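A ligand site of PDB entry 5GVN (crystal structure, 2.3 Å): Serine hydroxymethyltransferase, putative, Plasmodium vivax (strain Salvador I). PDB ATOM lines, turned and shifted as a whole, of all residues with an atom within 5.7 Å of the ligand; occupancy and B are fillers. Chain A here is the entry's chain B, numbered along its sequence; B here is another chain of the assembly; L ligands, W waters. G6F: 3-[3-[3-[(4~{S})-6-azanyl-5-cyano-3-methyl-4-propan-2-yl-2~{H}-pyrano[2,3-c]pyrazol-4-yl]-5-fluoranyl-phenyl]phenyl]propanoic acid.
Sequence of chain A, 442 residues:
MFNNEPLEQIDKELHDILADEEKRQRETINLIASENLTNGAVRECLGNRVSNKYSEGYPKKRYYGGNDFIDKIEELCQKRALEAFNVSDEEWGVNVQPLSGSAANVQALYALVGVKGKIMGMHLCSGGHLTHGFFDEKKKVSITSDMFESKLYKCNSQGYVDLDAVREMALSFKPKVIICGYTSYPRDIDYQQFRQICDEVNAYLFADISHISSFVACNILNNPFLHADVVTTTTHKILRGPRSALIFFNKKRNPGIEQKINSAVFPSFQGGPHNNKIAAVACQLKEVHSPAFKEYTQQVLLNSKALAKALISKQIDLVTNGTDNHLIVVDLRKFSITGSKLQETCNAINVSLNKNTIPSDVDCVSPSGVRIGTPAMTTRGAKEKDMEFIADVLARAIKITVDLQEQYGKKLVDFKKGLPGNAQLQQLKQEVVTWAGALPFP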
ATOM      1  N   HIS A 123      15.913  21.476  -1.706  1.00  0.00           N
ATOM      2  CA  HIS A 123      15.907  20.551  -0.592  1.00  0.00           C
ATOM      3  C   HIS A 123      16.244  19.122  -1.086  1.00  0.00           C
ATOM      4  O   HIS A 123      15.931  18.763  -2.236  1.00  0.00           O
ATOM      5  CB  HIS A 123      14.536  20.601   0.065  1.00  0.00           C
ATOM      6  CG  HIS A 123      14.485  20.047   1.438  1.00  0.00           C
ATOM      7  ND1 HIS A 123      14.489  18.695   1.678  1.00  0.00           N
ATOM      8  CD2 HIS A 123      14.383  20.656   2.641  1.00  0.00           C
ATOM      9  CE1 HIS A 123      14.406  18.490   2.977  1.00  0.00           C
ATOM     10  NE2 HIS A 123      14.350  19.660   3.590  1.00  0.00           N
ATOM     11  N   LEU A 124      16.888  18.320  -0.237  1.00  0.00           N
ATOM     12  CA  LEU A 124      17.261  16.935  -0.581  1.00  0.00           C
ATOM     13  C   LEU A 124      16.055  16.102  -1.024  1.00  0.00           C
ATOM     14  O   LEU A 124      16.097  15.486  -2.086  1.00  0.00           O
ATOM     15  CB  LEU A 124      17.954  16.242   0.600  1.00  0.00           C
ATOM     16  CG  LEU A 124      18.488  14.811   0.434  1.00  0.00           C
ATOM     17  CD1 LEU A 124      19.815  14.806  -0.300  1.00  0.00           C
ATOM     18  CD2 LEU A 124      18.651  14.084   1.766  1.00  0.00           C
ATOM     19  N   CYS A 125      15.033  16.083  -0.171  1.00  0.00           N
ATOM     20  CA  CYS A 125      13.681  15.510  -0.445  1.00  0.00           C
ATOM     21  C   CYS A 125      12.979  15.880  -1.750  1.00  0.00           C
ATOM     22  O   CYS A 125      12.127  15.114  -2.231  1.00  0.00           O
ATOM     23  CB  CYS A 125      12.729  15.838   0.719  1.00  0.00           C
ATOM     24  SG  CYS A 125      13.217  15.156   2.334  1.00  0.00           S
ATOM     25  N   GLY A 127      14.817  16.571  -4.542  1.00  0.00           N
ATOM     26  CA  GLY A 127      15.764  16.256  -5.608  1.00  0.00           C
ATOM     27  C   GLY A 127      17.057  17.046  -5.578  1.00  0.00           C
ATOM     28  O   GLY A 127      17.872  16.888  -6.463  1.00  0.00           O
ATOM     29  N   GLY A 128      17.251  17.880  -4.562  1.00  0.00           N
ATOM     30  CA  GLY A 128      18.512  18.570  -4.362  1.00  0.00           C
ATOM     31  C   GLY A 128      19.606  17.633  -3.881  1.00  0.00           C
ATOM     32  O   GLY A 128      19.338  16.492  -3.481  1.00  0.00           O
ATOM     33  N   HIS A 129      20.857  18.102  -3.975  1.00  0.00           N
ATOM     34  CA  HIS A 129      22.006  17.406  -3.429  1.00  0.00           C
ATOM     35  C   HIS A 129      22.284  17.832  -1.994  1.00  0.00           C
ATOM     36  O   HIS A 129      21.816  18.869  -1.518  1.00  0.00           O
ATOM     37  CB  HIS A 129      23.248  17.641  -4.281  1.00  0.00           C
ATOM     38  CG  HIS A 129      24.342  16.648  -4.018  1.00  0.00           C
ATOM     39  ND1 HIS A 129      25.567  17.008  -3.523  1.00  0.00           N
ATOM     40  CD2 HIS A 129      24.352  15.291  -4.101  1.00  0.00           C
ATOM     41  CE1 HIS A 129      26.303  15.925  -3.328  1.00  0.00           C
ATOM     42  NE2 HIS A 129      25.590  14.869  -3.697  1.00  0.00           N
ATOM     43  N   LEU A 130      23.064  16.995  -1.306  1.00  0.00           N
ATOM     44  CA  LEU A 130      23.576  17.280   0.048  1.00  0.00           C
ATOM     45  C   LEU A 130      24.393  18.578   0.122  1.00  0.00           C
ATOM     46  O   LEU A 130      24.192  19.384   1.021  1.00  0.00           O
ATOM     47  CB  LEU A 130      24.433  16.102   0.526  1.00  0.00           C
ATOM     48  CG  LEU A 130      23.671  14.789   0.670  1.00  0.00           C
ATOM     49  CD1 LEU A 130      24.639  13.632   0.757  1.00  0.00           C
ATOM     50  CD2 LEU A 130      22.785  14.839   1.904  1.00  0.00           C
ATOM     51  N   PHE A 134      21.902  21.179   2.522  1.00  0.00           N
ATOM     52  CA  PHE A 134      20.998  20.306   3.235  1.00  0.00           C
ATOM     53  C   PHE A 134      21.213  20.332   4.735  1.00  0.00           C
ATOM     54  O   PHE A 134      22.333  20.100   5.203  1.00  0.00           O
ATOM     55  CB  PHE A 134      21.119  18.851   2.786  1.00  0.00           C
ATOM     56  CG  PHE A 134      20.161  17.948   3.485  1.00  0.00           C
ATOM     57  CD1 PHE A 134      18.786  18.154   3.363  1.00  0.00           C
ATOM     58  CD2 PHE A 134      20.611  16.955   4.336  1.00  0.00           C
ATOM     59  CE1 PHE A 134      17.881  17.360   4.041  1.00  0.00           C
ATOM     60  CE2 PHE A 134      19.703  16.158   5.023  1.00  0.00           C
ATOM     61  CZ  PHE A 134      18.341  16.353   4.869  1.00  0.00           C
ATOM     62  N   ASP A 136      18.646  19.451   8.610  1.00  0.00           N
ATOM     63  CA  ASP A 136      17.496  18.807   9.240  1.00  0.00           C
ATOM     64  C   ASP A 136      17.274  19.509  10.590  1.00  0.00           C
ATOM     65  O   ASP A 136      18.223  20.044  11.150  1.00  0.00           O
ATOM     66  CB  ASP A 136      17.840  17.317   9.463  1.00  0.00           C
ATOM     67  CG  ASP A 136      16.640  16.422   9.618  1.00  0.00           C
ATOM     68  OD1 ASP A 136      15.489  16.914   9.763  1.00  0.00           O
ATOM     69  OD2 ASP A 136      16.851  15.192   9.607  1.00  0.00           O
ATOM     70  N   VAL A 141      23.309  18.608   8.519  1.00  0.00           N
ATOM     71  CA  VAL A 141      23.770  17.334   7.961  1.00  0.00           C
ATOM     72  C   VAL A 141      24.947  17.531   7.005  1.00  0.00           C
ATOM     73  O   VAL A 141      25.894  16.732   6.980  1.00  0.00           O
ATOM     74  CB  VAL A 141      22.589  16.602   7.270  1.00  0.00           C
ATOM     75  CG1 VAL A 141      23.040  15.400   6.459  1.00  0.00           C
ATOM     76  CG2 VAL A 141      21.549  16.182   8.310  1.00  0.00           C
ATOM     77  N   THR A 183      19.937  16.331  -8.191  1.00  0.00           N
ATOM     78  CA  THR A 183      20.368  14.914  -8.160  1.00  0.00           C
ATOM     79  C   THR A 183      19.314  13.957  -8.706  1.00  0.00           C
ATOM     80  O   THR A 183      19.650  13.012  -9.404  1.00  0.00           O
ATOM     81  CB  THR A 183      20.891  14.400  -6.794  1.00  0.00           C
ATOM     82  OG1 THR A 183      19.897  13.627  -6.117  1.00  0.00           O
ATOM     83  CG2 THR A 183      21.378  15.497  -5.947  1.00  0.00           C
ATOM     84  N   SER A 184      18.060  14.221  -8.401  1.00  0.00           N
ATOM     85  CA  SER A 184      16.952  13.368  -8.841  1.00  0.00           C
ATOM     86  C   SER A 184      15.825  14.252  -9.356  1.00  0.00           C
ATOM     87  O   SER A 184      14.714  14.257  -8.813  1.00  0.00           O
ATOM     88  CB  SER A 184      16.470  12.481  -7.670  1.00  0.00           C
ATOM     89  OG  SER A 184      17.557  12.101  -6.819  1.00  0.00           O
ATOM     90  N   ASN A 354      17.936   2.934  -6.748  1.00  0.00           N
ATOM     91  CA  ASN A 354      17.909   3.476  -5.420  1.00  0.00           C
ATOM     92  C   ASN A 354      16.535   3.997  -5.079  1.00  0.00           C
ATOM     93  O   ASN A 354      15.800   4.417  -5.942  1.00  0.00           O
ATOM     94  CB  ASN A 354      18.990   4.547  -5.193  1.00  0.00           C
ATOM     95  CG  ASN A 354      18.798   5.787  -6.043  1.00  0.00           C
ATOM     96  OD1 ASN A 354      19.258   5.853  -7.186  1.00  0.00           O
ATOM     97  ND2 ASN A 354      18.092   6.757  -5.495  1.00  0.00           N
ATOM     98  N   LYS A 355      16.217   3.899  -3.804  1.00  0.00           N
ATOM     99  CA  LYS A 355      15.069   4.554  -3.221  1.00  0.00           C
ATOM    100  C   LYS A 355      15.245   6.057  -3.314  1.00  0.00           C
ATOM    101  O   LYS A 355      16.362   6.580  -3.296  1.00  0.00           O
ATOM    102  CB  LYS A 355      14.863   4.134  -1.744  1.00  0.00           C
ATOM    103  CG  LYS A 355      16.137   4.172  -0.894  1.00  0.00           C
ATOM    104  CD  LYS A 355      15.858   4.261   0.611  1.00  0.00           C
ATOM    105  CE  LYS A 355      16.956   3.563   1.398  1.00  0.00           C
ATOM    106  NZ  LYS A 355      17.516   4.455   2.443  1.00  0.00           N
ATOM    107  N   ASN A 356      14.124   6.761  -3.388  1.00  0.00           N
ATOM    108  CA  ASN A 356      14.152   8.173  -3.688  1.00  0.00           C
ATOM    109  C   ASN A 356      12.864   8.811  -3.249  1.00  0.00           C
ATOM    110  O   ASN A 356      11.786   8.303  -3.542  1.00  0.00           O
ATOM    111  CB  ASN A 356      14.354   8.369  -5.200  1.00  0.00           C
ATOM    112  CG  ASN A 356      14.981   9.726  -5.535  1.00  0.00           C
ATOM    113  OD1 ASN A 356      16.185   9.820  -5.746  1.00  0.00           O
ATOM    114  ND2 ASN A 356      14.182  10.776  -5.501  1.00  0.00           N
ATOM    115  N   THR A 357      12.950   9.938  -2.560  1.00  0.00           N
ATOM    116  CA  THR A 357      11.767  10.703  -2.176  1.00  0.00           C
ATOM    117  C   THR A 357      10.888  11.128  -3.371  1.00  0.00           C
ATOM    118  O   THR A 357      11.353  11.174  -4.517  1.00  0.00           O
ATOM    119  CB  THR A 357      12.151  11.953  -1.387  1.00  0.00           C
ATOM    120  OG1 THR A 357      13.154  12.665  -2.120  1.00  0.00           O
ATOM    121  CG2 THR A 357      12.699  11.588  -0.009  1.00  0.00           C
ATOM    122  N   CYS A 364      12.745  12.445   4.543  1.00  0.00           N
ATOM    123  CA  CYS A 364      13.601  11.439   3.860  1.00  0.00           C
ATOM    124  C   CYS A 364      13.613  10.055   4.588  1.00  0.00           C
ATOM    125  O   CYS A 364      14.424   9.187   4.247  1.00  0.00           O
ATOM    126  CB  CYS A 364      15.030  11.979   3.710  1.00  0.00           C
ATOM    127  SG  CYS A 364      15.348  12.912   2.188  1.00  0.00           S
ATOM    128  N   VAL A 365      12.696   9.856   5.537  1.00  0.00           N
ATOM    129  CA  VAL A 365      12.724   8.721   6.470  1.00  0.00           C
ATOM    130  C   VAL A 365      12.167   7.466   5.778  1.00  0.00           C
ATOM    131  O   VAL A 365      12.766   6.395   5.838  1.00  0.00           O
ATOM    132  CB  VAL A 365      11.913   9.004   7.774  1.00  0.00           C
ATOM    133  CG1 VAL A 365      11.948   7.795   8.723  1.00  0.00           C
ATOM    134  CG2 VAL A 365      12.449  10.236   8.508  1.00  0.00           C
ATOM    135  N   PRO A 367      11.196   7.033   1.927  1.00  0.00           N
ATOM    136  CA  PRO A 367      10.957   7.481   0.546  1.00  0.00           C
ATOM    137  C   PRO A 367       9.988   6.558  -0.201  1.00  0.00           C
ATOM    138  O   PRO A 367      10.152   5.331  -0.173  1.00  0.00           O
ATOM    139  CB  PRO A 367      12.361   7.456  -0.094  1.00  0.00           C
ATOM    140  CG  PRO A 367      13.198   6.616   0.805  1.00  0.00           C
ATOM    141  CD  PRO A 367      12.613   6.762   2.176  1.00  0.00           C
ATOM    142  N   ARG A 371      14.409   5.793  -8.006  1.00  0.00           N
ATOM    143  CA  ARG A 371      14.952   6.467  -9.125  1.00  0.00           C
ATOM    144  C   ARG A 371      15.704   5.472 -10.008  1.00  0.00           C
ATOM    145  O   ARG A 371      16.525   4.668  -9.514  1.00  0.00           O
ATOM    146  CB  ARG A 371      15.860   7.566  -8.631  1.00  0.00           C
ATOM    147  CG  ARG A 371      16.546   8.379  -9.704  1.00  0.00           C
ATOM    148  CD  ARG A 371      17.595   9.264  -9.049  1.00  0.00           C
ATOM    149  NE  ARG A 371      18.762   8.486  -8.668  1.00  0.00           N
ATOM    150  CZ  ARG A 371      19.932   8.985  -8.328  1.00  0.00           C
ATOM    151  NH1 ARG A 371      20.153  10.301  -8.303  1.00  0.00           N
ATOM    152  NH2 ARG A 371      20.919   8.147  -8.017  1.00  0.00           N
ATOM    153  N   GLU B  56      27.674   5.413  -1.232  1.00  0.00           N
ATOM    154  CA  GLU B  56      27.576   6.411  -0.168  1.00  0.00           C
ATOM    155  C   GLU B  56      27.165   5.804   1.158  1.00  0.00           C
ATOM    156  O   GLU B  56      26.250   5.001   1.218  1.00  0.00           O
ATOM    157  CB  GLU B  56      26.580   7.497  -0.540  1.00  0.00           C
ATOM    158  CG  GLU B  56      26.984   8.342  -1.745  1.00  0.00           C
ATOM    159  CD  GLU B  56      25.927   9.352  -2.121  1.00  0.00           C
ATOM    160  OE1 GLU B  56      24.969   8.986  -2.826  1.00  0.00           O
ATOM    161  OE2 GLU B  56      26.035  10.498  -1.689  1.00  0.00           O
ATOM    162  N   TYR B  63      23.513   3.341   1.479  1.00  0.00           N
ATOM    163  CA  TYR B  63      22.263   3.869   0.936  1.00  0.00           C
ATOM    164  C   TYR B  63      21.752   2.919  -0.130  1.00  0.00           C
ATOM    165  O   TYR B  63      20.537   2.705  -0.199  1.00  0.00           O
ATOM    166  CB  TYR B  63      22.403   5.335   0.468  1.00  0.00           C
ATOM    167  CG  TYR B  63      22.251   6.256   1.668  1.00  0.00           C
ATOM    168  CD1 TYR B  63      23.326   6.514   2.489  1.00  0.00           C
ATOM    169  CD2 TYR B  63      21.024   6.744   2.035  1.00  0.00           C
ATOM    170  CE1 TYR B  63      23.187   7.281   3.633  1.00  0.00           C
ATOM    171  CE2 TYR B  63      20.860   7.515   3.183  1.00  0.00           C
ATOM    172  CZ  TYR B  63      21.954   7.781   3.980  1.00  0.00           C
ATOM    173  OH  TYR B  63      21.856   8.547   5.126  1.00  0.00           O
ATOM    174  N   TYR B  64      22.650   2.336  -0.922  1.00  0.00           N
ATOM    175  CA  TYR B  64      22.282   1.413  -2.012  1.00  0.00           C
ATOM    176  C   TYR B  64      22.656  -0.038  -1.738  1.00  0.00           C
ATOM    177  O   TYR B  64      23.538  -0.298  -0.941  1.00  0.00           O
ATOM    178  CB  TYR B  64      22.968   1.781  -3.334  1.00  0.00           C
ATOM    179  CG  TYR B  64      22.875   3.218  -3.762  1.00  0.00           C
ATOM    180  CD1 TYR B  64      22.002   4.121  -3.163  1.00  0.00           C
ATOM    181  CD2 TYR B  64      23.660   3.678  -4.827  1.00  0.00           C
ATOM    182  CE1 TYR B  64      21.929   5.427  -3.585  1.00  0.00           C
ATOM    183  CE2 TYR B  64      23.591   4.998  -5.266  1.00  0.00           C
ATOM    184  CZ  TYR B  64      22.722   5.876  -4.639  1.00  0.00           C
ATOM    185  OH  TYR B  64      22.659   7.184  -5.058  1.00  0.00           O
ATOM    186  N   PHE B 266      31.352  11.598   5.747  1.00  0.00           N
ATOM    187  CA  PHE B 266      30.090  11.557   4.986  1.00  0.00           C
ATOM    188  C   PHE B 266      28.924  11.527   5.954  1.00  0.00           C
ATOM    189  O   PHE B 266      28.896  10.671   6.821  1.00  0.00           O
ATOM    190  CB  PHE B 266      30.015  10.321   4.102  1.00  0.00           C
ATOM    191  CG  PHE B 266      28.643  10.097   3.531  1.00  0.00           C
ATOM    192  CD1 PHE B 266      28.232  10.777   2.380  1.00  0.00           C
ATOM    193  CD2 PHE B 266      27.739   9.231   4.149  1.00  0.00           C
ATOM    194  CE1 PHE B 266      26.976  10.581   1.862  1.00  0.00           C
ATOM    195  CE2 PHE B 266      26.491   9.029   3.611  1.00  0.00           C
ATOM    196  CZ  PHE B 266      26.103   9.693   2.462  1.00  0.00           C
ATOM    197  N   PRO B 267      27.907  12.375   5.787  1.00  0.00           N
ATOM    198  CA  PRO B 267      27.680  13.243   4.631  1.00  0.00           C
ATOM    199  C   PRO B 267      28.070  14.706   4.807  1.00  0.00           C
ATOM    200  O   PRO B 267      27.700  15.530   3.962  1.00  0.00           O
ATOM    201  CB  PRO B 267      26.156  13.153   4.465  1.00  0.00           C
ATOM    202  CG  PRO B 267      25.680  13.027   5.867  1.00  0.00           C
ATOM    203  CD  PRO B 267      26.649  12.077   6.500  1.00  0.00           C
HETATM  204  O58 G6F L   1      18.005   9.586   8.188  1.00  0.00           O
HETATM  205  C48 G6F L   1      18.761  10.572   7.941  1.00  0.00           C
HETATM  206  O55 G6F L   1      19.840  10.783   8.559  1.00  0.00           O
HETATM  207  C47 G6F L   1      18.298  11.494   6.823  1.00  0.00           C
HETATM  208  C46 G6F L   1      19.376  12.411   6.206  1.00  0.00           C
HETATM  209  C42 G6F L   1      20.041  11.833   4.969  1.00  0.00           C
HETATM  210  C41 G6F L   1      19.297  11.342   3.891  1.00  0.00           C
HETATM  211  C43 G6F L   1      21.437  11.814   4.939  1.00  0.00           C
HETATM  212  C44 G6F L   1      22.086  11.313   3.834  1.00  0.00           C
HETATM  213  C45 G6F L   1      21.342  10.810   2.763  1.00  0.00           C
HETATM  214  C34 G6F L   1      19.945  10.822   2.769  1.00  0.00           C
HETATM  215  C20 G6F L   1      19.237  10.264   1.589  1.00  0.00           C
HETATM  216  C19 G6F L   1      18.191   9.347   1.711  1.00  0.00           C
HETATM  217  C18 G6F L   1      17.573   8.835   0.559  1.00  0.00           C
HETATM  218  F35 G6F L   1      16.581   7.956   0.663  1.00  0.00           F
HETATM  219  C17 G6F L   1      17.990   9.254  -0.693  1.00  0.00           C
HETATM  220  C21 G6F L   1      19.634  10.673   0.307  1.00  0.00           C
HETATM  221  C16 G6F L   1      19.038  10.178  -0.856  1.00  0.00           C
HETATM  222  C4  G6F L   1      19.470  10.626  -2.257  1.00  0.00           C
HETATM  223  C14 G6F L   1      19.401   9.544  -3.359  1.00  0.00           C
HETATM  224  C36 G6F L   1      19.975   9.967  -4.724  1.00  0.00           C
HETATM  225  C15 G6F L   1      20.054   8.202  -2.984  1.00  0.00           C
HETATM  226  C3  G6F L   1      18.521  11.761  -2.666  1.00  0.00           C
HETATM  227  C8  G6F L   1      17.270  11.524  -2.591  1.00  0.00           C
HETATM  228  N9  G6F L   1      16.127  11.314  -2.530  1.00  0.00           N
HETATM  229  C2  G6F L   1      18.975  12.961  -3.103  1.00  0.00           C
HETATM  230  N7  G6F L   1      18.189  13.962  -3.485  1.00  0.00           N
HETATM  231  C5  G6F L   1      20.876  11.113  -2.191  1.00  0.00           C
HETATM  232  C10 G6F L   1      22.151  10.526  -1.688  1.00  0.00           C
HETATM  233  C13 G6F L   1      22.420   9.184  -1.043  1.00  0.00           C
HETATM  234  N11 G6F L   1      23.086  11.476  -1.910  1.00  0.00           N
HETATM  235  N12 G6F L   1      22.607  12.665  -2.495  1.00  0.00           N
HETATM  236  C6  G6F L   1      21.304  12.418  -2.665  1.00  0.00           C
HETATM  237  O1  G6F L   1      20.387  13.261  -3.211  1.00  0.00           O
HETATM  238  O   HOH W   1      19.258   8.600   5.827  1.00  0.00           O
HETATM  239  O   HOH W   2      14.647  13.413  -4.380  1.00  0.00           O
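The side-chain carboxylate (OE2) of Glu 56 of chain B is in hydrogen-bond range of a nitrogen (N11) of the ligand (3.1 Å). The side-chain hydroxyl (OG1) of Thr 357 lies within hydrogen-bond range of a nitrogen (N9) of the ligand (3.3 Å). O of Gly 128 lies within hydrogen-bond range of N7 of the ligand. The backbone NH of Thr 357 is in hydrogen-bond range of a nitrogen (N9) of the ligand (3.5 Å). O of Leu 124 lies within hydrogen-bond range of N7 of the ligand (2.9 Å). O1 of the ligand sits at hydrogen-bond distance from OG1 of Thr 183.
The backbone carbonyl oxygen (O) of Asn 354 is in hydrogen-bond range of the backbone NH (N) of Arg 371 (2.8 Å). The side-chain hydroxyl (OG) of Ser 184 sits at hydrogen-bond distance from the side-chain hydroxyl (OG1) of Thr 183 (2.9 Å). The backbone NH (N) of Tyr 63 of chain B sits at hydrogen-bond distance from the backbone carbonyl oxygen (O) of Glu 56 of chain B (3.2 Å). The side-chain amide oxygen (OD1) of Asn 356 is in hydrogen-bond range of the side-chain hydroxyl (OG) of Ser 184 (2.9 Å). O of Cys 125 lies within hydrogen-bond range of OG1 of Thr 357 (2.7 Å). The guanidinium group (NH1) of Arg 371 lies within hydrogen-bond range of the side-chain hydroxyl (OG) of Ser 184, 3.5 Å away. The backbone NH (N) of Gly 128 is in hydrogen-bond range of the backbone carbonyl oxygen (O) of His 123 (2.8 Å). O of Gly 127 is in hydrogen-bond range of N of Thr 183.
Gly 127 touches the ligand (C to N7, 3.9 Å). CD2 of His 129 touches N12 of the ligand, at 3.5 Å. CD1 of Leu 130 touches N11 of the ligand, at 3.8 Å. Phe 134 touches the ligand (CE2 to C46, 3.9 Å). OG of Ser 184 touches C36 of the ligand, at 3.8 Å. Asn 354 touches the ligand. Lys 355 touches the ligand (CD to F35, 3.8 Å). Asn 356 touches the ligand. CG of Pro 367 touches F35 of the ligand (3.6 Å). Arg 371 touches the ligand (NH1 to C36, 3.6 Å). OH of Tyr 63 of chain B touches C44 of the ligand (3.1 Å). Tyr 64 of chain B touches the ligand (CE1 to C15, 3.4 Å). Of the 25 residues printed, 17 come within 4 Å of the ligand. The nearest printed residue that does not touch the ligand is Val 141 (4.2 Å).
Water W1 lies within hydrogen-bond range of OH of Tyr 63 of chain B (2.7 Å) and O58 of the ligand (2.8 Å). Water W2 lies within hydrogen-bond range of the side-chain hydroxyl (OG1) of Thr 357 (2.8 Å), the side-chain amide nitrogen (ND2) of Asn 356 (2.9 Å), a nitrogen (N9) of the ligand (3.2 Å), the backbone NH (N) of Gly 127 (3.2 Å) and the backbone carbonyl oxygen (O) of Leu 124 (3.4 Å).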
